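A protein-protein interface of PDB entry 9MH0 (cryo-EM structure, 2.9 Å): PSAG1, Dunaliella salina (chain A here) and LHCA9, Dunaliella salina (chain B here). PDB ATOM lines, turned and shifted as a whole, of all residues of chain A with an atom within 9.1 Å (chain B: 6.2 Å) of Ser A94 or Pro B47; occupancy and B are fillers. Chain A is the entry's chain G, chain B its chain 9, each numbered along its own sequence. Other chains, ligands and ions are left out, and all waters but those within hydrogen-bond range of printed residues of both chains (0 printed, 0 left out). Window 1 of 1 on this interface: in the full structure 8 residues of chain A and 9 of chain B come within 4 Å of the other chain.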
ATOM      1  N   ARG A  88      29.231 -29.772  23.119  1.00  0.00           N
ATOM      2  CA  ARG A  88      28.632 -29.291  21.878  1.00  0.00           C
ATOM      3  C   ARG A  88      28.835 -27.797  21.680  1.00  0.00           C
ATOM      4  O   ARG A  88      28.725 -27.317  20.548  1.00  0.00           O
ATOM      5  CB  ARG A  88      27.139 -29.620  21.834  1.00  0.00           C
ATOM      6  CG  ARG A  88      26.773 -30.976  22.403  1.00  0.00           C
ATOM      7  CD  ARG A  88      26.584 -32.017  21.308  1.00  0.00           C
ATOM      8  NE  ARG A  88      25.804 -33.163  21.766  1.00  0.00           N
ATOM      9  CZ  ARG A  88      24.491 -33.164  21.941  1.00  0.00           C
ATOM     10  NH1 ARG A  88      23.754 -32.099  21.676  1.00  0.00           N
ATOM     11  NH2 ARG A  88      23.897 -34.269  22.386  1.00  0.00           N
ATOM     12  N   LYS A  91      31.841 -27.583  19.698  1.00  0.00           N
ATOM     13  CA  LYS A  91      31.643 -28.098  18.355  1.00  0.00           C
ATOM     14  C   LYS A  91      31.365 -26.943  17.393  1.00  0.00           C
ATOM     15  O   LYS A  91      30.833 -25.906  17.802  1.00  0.00           O
ATOM     16  CB  LYS A  91      30.487 -29.099  18.333  1.00  0.00           C
ATOM     17  CG  LYS A  91      30.935 -30.551  18.375  1.00  0.00           C
ATOM     18  CD  LYS A  91      29.906 -31.433  19.060  1.00  0.00           C
ATOM     19  CE  LYS A  91      30.574 -32.539  19.860  1.00  0.00           C
ATOM     20  NZ  LYS A  91      29.584 -33.466  20.468  1.00  0.00           N
ATOM     21  N   PRO A  92      31.732 -27.086  16.117  1.00  0.00           N
ATOM     22  CA  PRO A  92      31.534 -25.991  15.161  1.00  0.00           C
ATOM     23  C   PRO A  92      30.060 -25.672  14.953  1.00  0.00           C
ATOM     24  O   PRO A  92      29.176 -26.512  15.138  1.00  0.00           O
ATOM     25  CB  PRO A  92      32.172 -26.519  13.871  1.00  0.00           C
ATOM     26  CG  PRO A  92      33.147 -27.543  14.327  1.00  0.00           C
ATOM     27  CD  PRO A  92      32.528 -28.181  15.532  1.00  0.00           C
ATOM     28  N   ALA A  93      29.807 -24.425  14.567  1.00  0.00           N
ATOM     29  CA  ALA A  93      28.451 -23.915  14.413  1.00  0.00           C
ATOM     30  C   ALA A  93      27.782 -24.573  13.205  1.00  0.00           C
ATOM     31  O   ALA A  93      28.390 -25.341  12.457  1.00  0.00           O
ATOM     32  CB  ALA A  93      28.475 -22.396  14.294  1.00  0.00           C
ATOM     33  N   SER A  94      26.502 -24.267  13.006  1.00  0.00           N
ATOM     34  CA  SER A  94      25.729 -24.877  11.935  1.00  0.00           C
ATOM     35  C   SER A  94      25.571 -23.985  10.712  1.00  0.00           C
ATOM     36  O   SER A  94      25.127 -24.473   9.667  1.00  0.00           O
ATOM     37  CB  SER A  94      24.341 -25.277  12.445  1.00  0.00           C
ATOM     38  OG  SER A  94      24.441 -26.244  13.474  1.00  0.00           O
ATOM     39  N   PHE A  95      25.907 -22.700  10.815  1.00  0.00           N
ATOM     40  CA  PHE A  95      25.745 -21.760   9.716  1.00  0.00           C
ATOM     41  C   PHE A  95      27.067 -21.381   9.057  1.00  0.00           C
ATOM     42  O   PHE A  95      27.097 -20.457   8.237  1.00  0.00           O
ATOM     43  CB  PHE A  95      25.007 -20.506  10.204  1.00  0.00           C
ATOM     44  CG  PHE A  95      25.881 -19.502  10.899  1.00  0.00           C
ATOM     45  CD1 PHE A  95      26.440 -19.781  12.133  1.00  0.00           C
ATOM     46  CD2 PHE A  95      26.119 -18.262  10.324  1.00  0.00           C
ATOM     47  CE1 PHE A  95      27.235 -18.854  12.773  1.00  0.00           C
ATOM     48  CE2 PHE A  95      26.913 -17.329  10.962  1.00  0.00           C
ATOM     49  CZ  PHE A  95      27.471 -17.627  12.187  1.00  0.00           C
ATOM     50  N   VAL A  96      28.154 -22.084   9.374  1.00  0.00           N
ATOM     51  CA  VAL A  96      29.477 -21.758   8.855  1.00  0.00           C
ATOM     52  C   VAL A  96      29.982 -22.772   7.843  1.00  0.00           C
ATOM     53  O   VAL A  96      31.064 -22.572   7.273  1.00  0.00           O
ATOM     54  CB  VAL A  96      30.498 -21.590   9.996  1.00  0.00           C
ATOM     55  CG1 VAL A  96      29.982 -20.601  11.028  1.00  0.00           C
ATOM     56  CG2 VAL A  96      30.800 -22.934  10.641  1.00  0.00           C
ATOM     57  N   GLU A  97      29.242 -23.856   7.597  1.00  0.00           N
ATOM     58  CA  GLU A  97      29.666 -24.879   6.647  1.00  0.00           C
ATOM     59  C   GLU A  97      28.607 -25.180   5.592  1.00  0.00           C
ATOM     60  O   GLU A  97      28.690 -26.224   4.932  1.00  0.00           O
ATOM     61  CB  GLU A  97      30.050 -26.170   7.388  1.00  0.00           C
ATOM     62  CG  GLU A  97      28.884 -26.917   8.043  1.00  0.00           C
ATOM     63  CD  GLU A  97      28.529 -26.401   9.424  1.00  0.00           C
ATOM     64  OE1 GLU A  97      28.201 -27.234  10.297  1.00  0.00           O
ATOM     65  OE2 GLU A  97      28.559 -25.172   9.643  1.00  0.00           O
ATOM     66  N   THR A  98      27.641 -24.284   5.387  1.00  0.00           N
ATOM     67  CA  THR A  98      26.490 -24.596   4.546  1.00  0.00           C
ATOM     68  C   THR A  98      26.734 -24.367   3.061  1.00  0.00           C
ATOM     69  O   THR A  98      25.754 -24.344   2.307  1.00  0.00           O
ATOM     70  CB  THR A  98      25.279 -23.770   4.985  1.00  0.00           C
ATOM     71  OG1 THR A  98      25.338 -22.471   4.384  1.00  0.00           O
ATOM     72  CG2 THR A  98      25.251 -23.623   6.495  1.00  0.00           C
ATOM     73  N   LYS A  99      27.997 -24.217   2.631  1.00  0.00           N
ATOM     74  CA  LYS A  99      28.384 -24.002   1.233  1.00  0.00           C
ATOM     75  C   LYS A  99      27.672 -22.732   0.770  1.00  0.00           C
ATOM     76  O   LYS A  99      26.640 -22.791   0.089  1.00  0.00           O
ATOM     77  CB  LYS A  99      28.093 -25.264   0.382  1.00  0.00           C
ATOM     78  CG  LYS A  99      28.042 -25.189  -1.177  1.00  0.00           C
ATOM     79  CD  LYS A  99      29.096 -24.272  -1.820  1.00  0.00           C
ATOM     80  CE  LYS A  99      28.603 -23.716  -3.153  1.00  0.00           C
ATOM     81  NZ  LYS A  99      27.733 -22.520  -2.982  1.00  0.00           N
ATOM     82  N   ILE A 109      30.789 -15.385   7.689  1.00  0.00           N
ATOM     83  CA  ILE A 109      31.793 -15.051   8.693  1.00  0.00           C
ATOM     84  C   ILE A 109      32.970 -14.318   8.055  1.00  0.00           C
ATOM     85  O   ILE A 109      33.495 -13.349   8.619  1.00  0.00           O
ATOM     86  CB  ILE A 109      32.239 -16.327   9.430  1.00  0.00           C
ATOM     87  CG1 ILE A 109      31.071 -16.907  10.226  1.00  0.00           C
ATOM     88  CG2 ILE A 109      33.388 -16.037  10.372  1.00  0.00           C
ATOM     89  CD1 ILE A 109      30.486 -15.938  11.225  1.00  0.00           C
ATOM     90  N   VAL B  43      19.664 -22.164   3.193  1.00  0.00           N
ATOM     91  CA  VAL B  43      19.994 -23.405   3.887  1.00  0.00           C
ATOM     92  C   VAL B  43      20.853 -23.131   5.112  1.00  0.00           C
ATOM     93  O   VAL B  43      21.996 -22.677   4.997  1.00  0.00           O
ATOM     94  CB  VAL B  43      20.687 -24.389   2.936  1.00  0.00           C
ATOM     95  CG1 VAL B  43      21.062 -25.648   3.680  1.00  0.00           C
ATOM     96  CG2 VAL B  43      19.771 -24.708   1.761  1.00  0.00           C
ATOM     97  N   ILE B  44      20.302 -23.415   6.292  1.00  0.00           N
ATOM     98  CA  ILE B  44      21.028 -23.377   7.561  1.00  0.00           C
ATOM     99  C   ILE B  44      20.452 -24.460   8.471  1.00  0.00           C
ATOM    100  O   ILE B  44      19.668 -24.155   9.382  1.00  0.00           O
ATOM    101  CB  ILE B  44      20.955 -21.988   8.213  1.00  0.00           C
ATOM    102  CG1 ILE B  44      19.514 -21.589   8.552  1.00  0.00           C
ATOM    103  CG2 ILE B  44      21.558 -20.932   7.296  1.00  0.00           C
ATOM    104  CD1 ILE B  44      19.108 -21.775   9.988  1.00  0.00           C
ATOM    105  N   PRO B  45      20.821 -25.726   8.278  1.00  0.00           N
ATOM    106  CA  PRO B  45      20.133 -26.831   8.967  1.00  0.00           C
ATOM    107  C   PRO B  45      20.481 -26.882  10.443  1.00  0.00           C
ATOM    108  O   PRO B  45      21.661 -26.982  10.815  1.00  0.00           O
ATOM    109  CB  PRO B  45      20.647 -28.079   8.235  1.00  0.00           C
ATOM    110  CG  PRO B  45      21.952 -27.663   7.651  1.00  0.00           C
ATOM    111  CD  PRO B  45      21.826 -26.211   7.315  1.00  0.00           C
ATOM    112  N   PRO B  46      19.481 -26.819  11.319  1.00  0.00           N
ATOM    113  CA  PRO B  46      19.739 -26.925  12.756  1.00  0.00           C
ATOM    114  C   PRO B  46      19.691 -28.371  13.221  1.00  0.00           C
ATOM    115  O   PRO B  46      18.749 -29.112  12.898  1.00  0.00           O
ATOM    116  CB  PRO B  46      18.602 -26.100  13.373  1.00  0.00           C
ATOM    117  CG  PRO B  46      17.484 -26.180  12.368  1.00  0.00           C
ATOM    118  CD  PRO B  46      18.063 -26.550  11.022  1.00  0.00           C
ATOM    119  N   PRO B  47      20.694 -28.813  13.983  1.00  0.00           N
ATOM    120  CA  PRO B  47      20.682 -30.216  14.441  1.00  0.00           C
ATOM    121  C   PRO B  47      19.674 -30.483  15.545  1.00  0.00           C
ATOM    122  O   PRO B  47      19.004 -31.522  15.523  1.00  0.00           O
ATOM    123  CB  PRO B  47      22.127 -30.435  14.912  1.00  0.00           C
ATOM    124  CG  PRO B  47      22.601 -29.077  15.312  1.00  0.00           C
ATOM    125  CD  PRO B  47      21.905 -28.094  14.408  1.00  0.00           C
ATOM    126  N   HIS B  48      19.547 -29.579  16.513  1.00  0.00           N
ATOM    127  CA  HIS B  48      18.679 -29.789  17.664  1.00  0.00           C
ATOM    128  C   HIS B  48      17.316 -29.121  17.520  1.00  0.00           C
ATOM    129  O   HIS B  48      16.518 -29.172  18.462  1.00  0.00           O
ATOM    130  CB  HIS B  48      19.368 -29.292  18.942  1.00  0.00           C
ATOM    131  CG  HIS B  48      19.702 -27.831  18.925  1.00  0.00           C
ATOM    132  ND1 HIS B  48      20.678 -27.297  18.112  1.00  0.00           N
ATOM    133  CD2 HIS B  48      19.196 -26.795  19.635  1.00  0.00           C
ATOM    134  CE1 HIS B  48      20.756 -25.995  18.315  1.00  0.00           C
ATOM    135  NE2 HIS B  48      19.867 -25.665  19.234  1.00  0.00           N
ATOM    136  N   LEU B  49      17.030 -28.500  16.381  1.00  0.00           N
ATOM    137  CA  LEU B  49      15.737 -27.872  16.117  1.00  0.00           C
ATOM    138  C   LEU B  49      15.112 -28.596  14.926  1.00  0.00           C
ATOM    139  O   LEU B  49      15.316 -28.217  13.772  1.00  0.00           O
ATOM    140  CB  LEU B  49      15.891 -26.376  15.853  1.00  0.00           C
ATOM    141  CG  LEU B  49      16.677 -25.584  16.900  1.00  0.00           C
ATOM    142  CD1 LEU B  49      16.681 -24.103  16.558  1.00  0.00           C
ATOM    143  CD2 LEU B  49      16.102 -25.812  18.287  1.00  0.00           C
ATOM    144  N   ASN B  50      14.344 -29.647  15.221  1.00  0.00           N
ATOM    145  CA  ASN B  50      13.728 -30.440  14.162  1.00  0.00           C
ATOM    146  C   ASN B  50      12.619 -29.667  13.458  1.00  0.00           C
ATOM    147  O   ASN B  50      12.495 -29.732  12.231  1.00  0.00           O
ATOM    148  CB  ASN B  50      13.190 -31.748  14.736  1.00  0.00           C
ATOM    149  CG  ASN B  50      12.625 -31.580  16.133  1.00  0.00           C
ATOM    150  OD1 ASN B  50      12.354 -30.464  16.572  1.00  0.00           O
ATOM    151  ND2 ASN B  50      12.450 -32.691  16.839  1.00  0.00           N
ATOM    152  N   ASP B  60      19.861 -20.564  15.543  1.00  0.00           N
ATOM    153  CA  ASP B  60      20.832 -20.851  16.599  1.00  0.00           C
ATOM    154  C   ASP B  60      22.228 -20.830  15.992  1.00  0.00           C
ATOM    155  O   ASP B  60      22.852 -21.876  15.779  1.00  0.00           O
ATOM    156  CB  ASP B  60      20.540 -22.196  17.263  1.00  0.00           C
ATOM    157  CG  ASP B  60      20.854 -22.189  18.748  1.00  0.00           C
ATOM    158  OD1 ASP B  60      21.683 -21.361  19.176  1.00  0.00           O
ATOM    159  OD2 ASP B  60      20.278 -23.017  19.484  1.00  0.00           O
ATOM    160  N   PRO B  61      22.749 -19.636  15.683  1.00  0.00           N
ATOM    161  CA  PRO B  61      24.085 -19.559  15.071  1.00  0.00           C
ATOM    162  C   PRO B  61      25.211 -19.937  16.011  1.00  0.00           C
ATOM    163  O   PRO B  61      26.310 -20.246  15.537  1.00  0.00           O
ATOM    164  CB  PRO B  61      24.190 -18.090  14.648  1.00  0.00           C
ATOM    165  CG  PRO B  61      23.316 -17.378  15.616  1.00  0.00           C
ATOM    166  CD  PRO B  61      22.161 -18.298  15.872  1.00  0.00           C
ATOM    167  N   LEU B  66      21.290 -26.901  23.199  1.00  0.00           N
ATOM    168  CA  LEU B  66      21.430 -28.326  22.905  1.00  0.00           C
ATOM    169  C   LEU B  66      20.783 -29.199  23.974  1.00  0.00           C
ATOM    170  O   LEU B  66      20.179 -30.225  23.642  1.00  0.00           O
ATOM    171  CB  LEU B  66      22.904 -28.707  22.742  1.00  0.00           C
ATOM    172  CG  LEU B  66      23.713 -28.252  21.517  1.00  0.00           C
ATOM    173  CD1 LEU B  66      22.996 -28.627  20.225  1.00  0.00           C
ATOM    174  CD2 LEU B  66      24.089 -26.778  21.533  1.00  0.00           C
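The backbone carbonyl oxygen of Val B43 lies within hydrogen-bond range of the side-chain hydroxyl of Thr A98 (3.4 Å).
Arg A88 touches Leu B66. Pro B61 touches Ala A93. CB of Ser A94 touches O of Pro B45, at 3.6 Å. OG of Ser A94 touches CD of Pro B47, 3.3 Å away. CE1 of Phe A95 touches O of Pro B61 (3.2 Å).
Of chain B, only Pro B45 and Pro B47 come within 4 Å of Ser A94. Pro B47 touches just one residue of chain A: Ser A94 (3.3 Å). Of the printed residues of chain B, Ala A93 touches Pro B61. Of the printed residues of chain B, Arg A88 touches Leu B66 (3.7 Å). Of the printed residues of chain B, Thr A98 touches Val B43 (3.4 Å). Of the printed residues of chain B, Phe A95 touches Pro B61 (3.2 Å). Of the printed residues of chain A, Pro B45 touches Ser A94 (3.6 Å). The nearest printed residue of chain B that does not touch Ser A94 is Ile B44 (4.7 Å). The nearest residue of chain A that does not touch Pro B47 is Ala A93 (7.0 Å). The nearest printed residue of chain A that does not touch Val B43 is Ser A94 (5.9 Å).
Hydrophobic or aromatic side chains of chain B that line the printed part of chain A: Pro B47, Pro B61 and Leu B66. Hydrophobic or aromatic side chains of chain A within 4 Å of the printed part of chain B: Ala A93 and Phe A95. Among the printed residues, no Asp or Glu carboxylate lies within 4 Å of a Lys or Arg side-chain nitrogen of the other chain.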
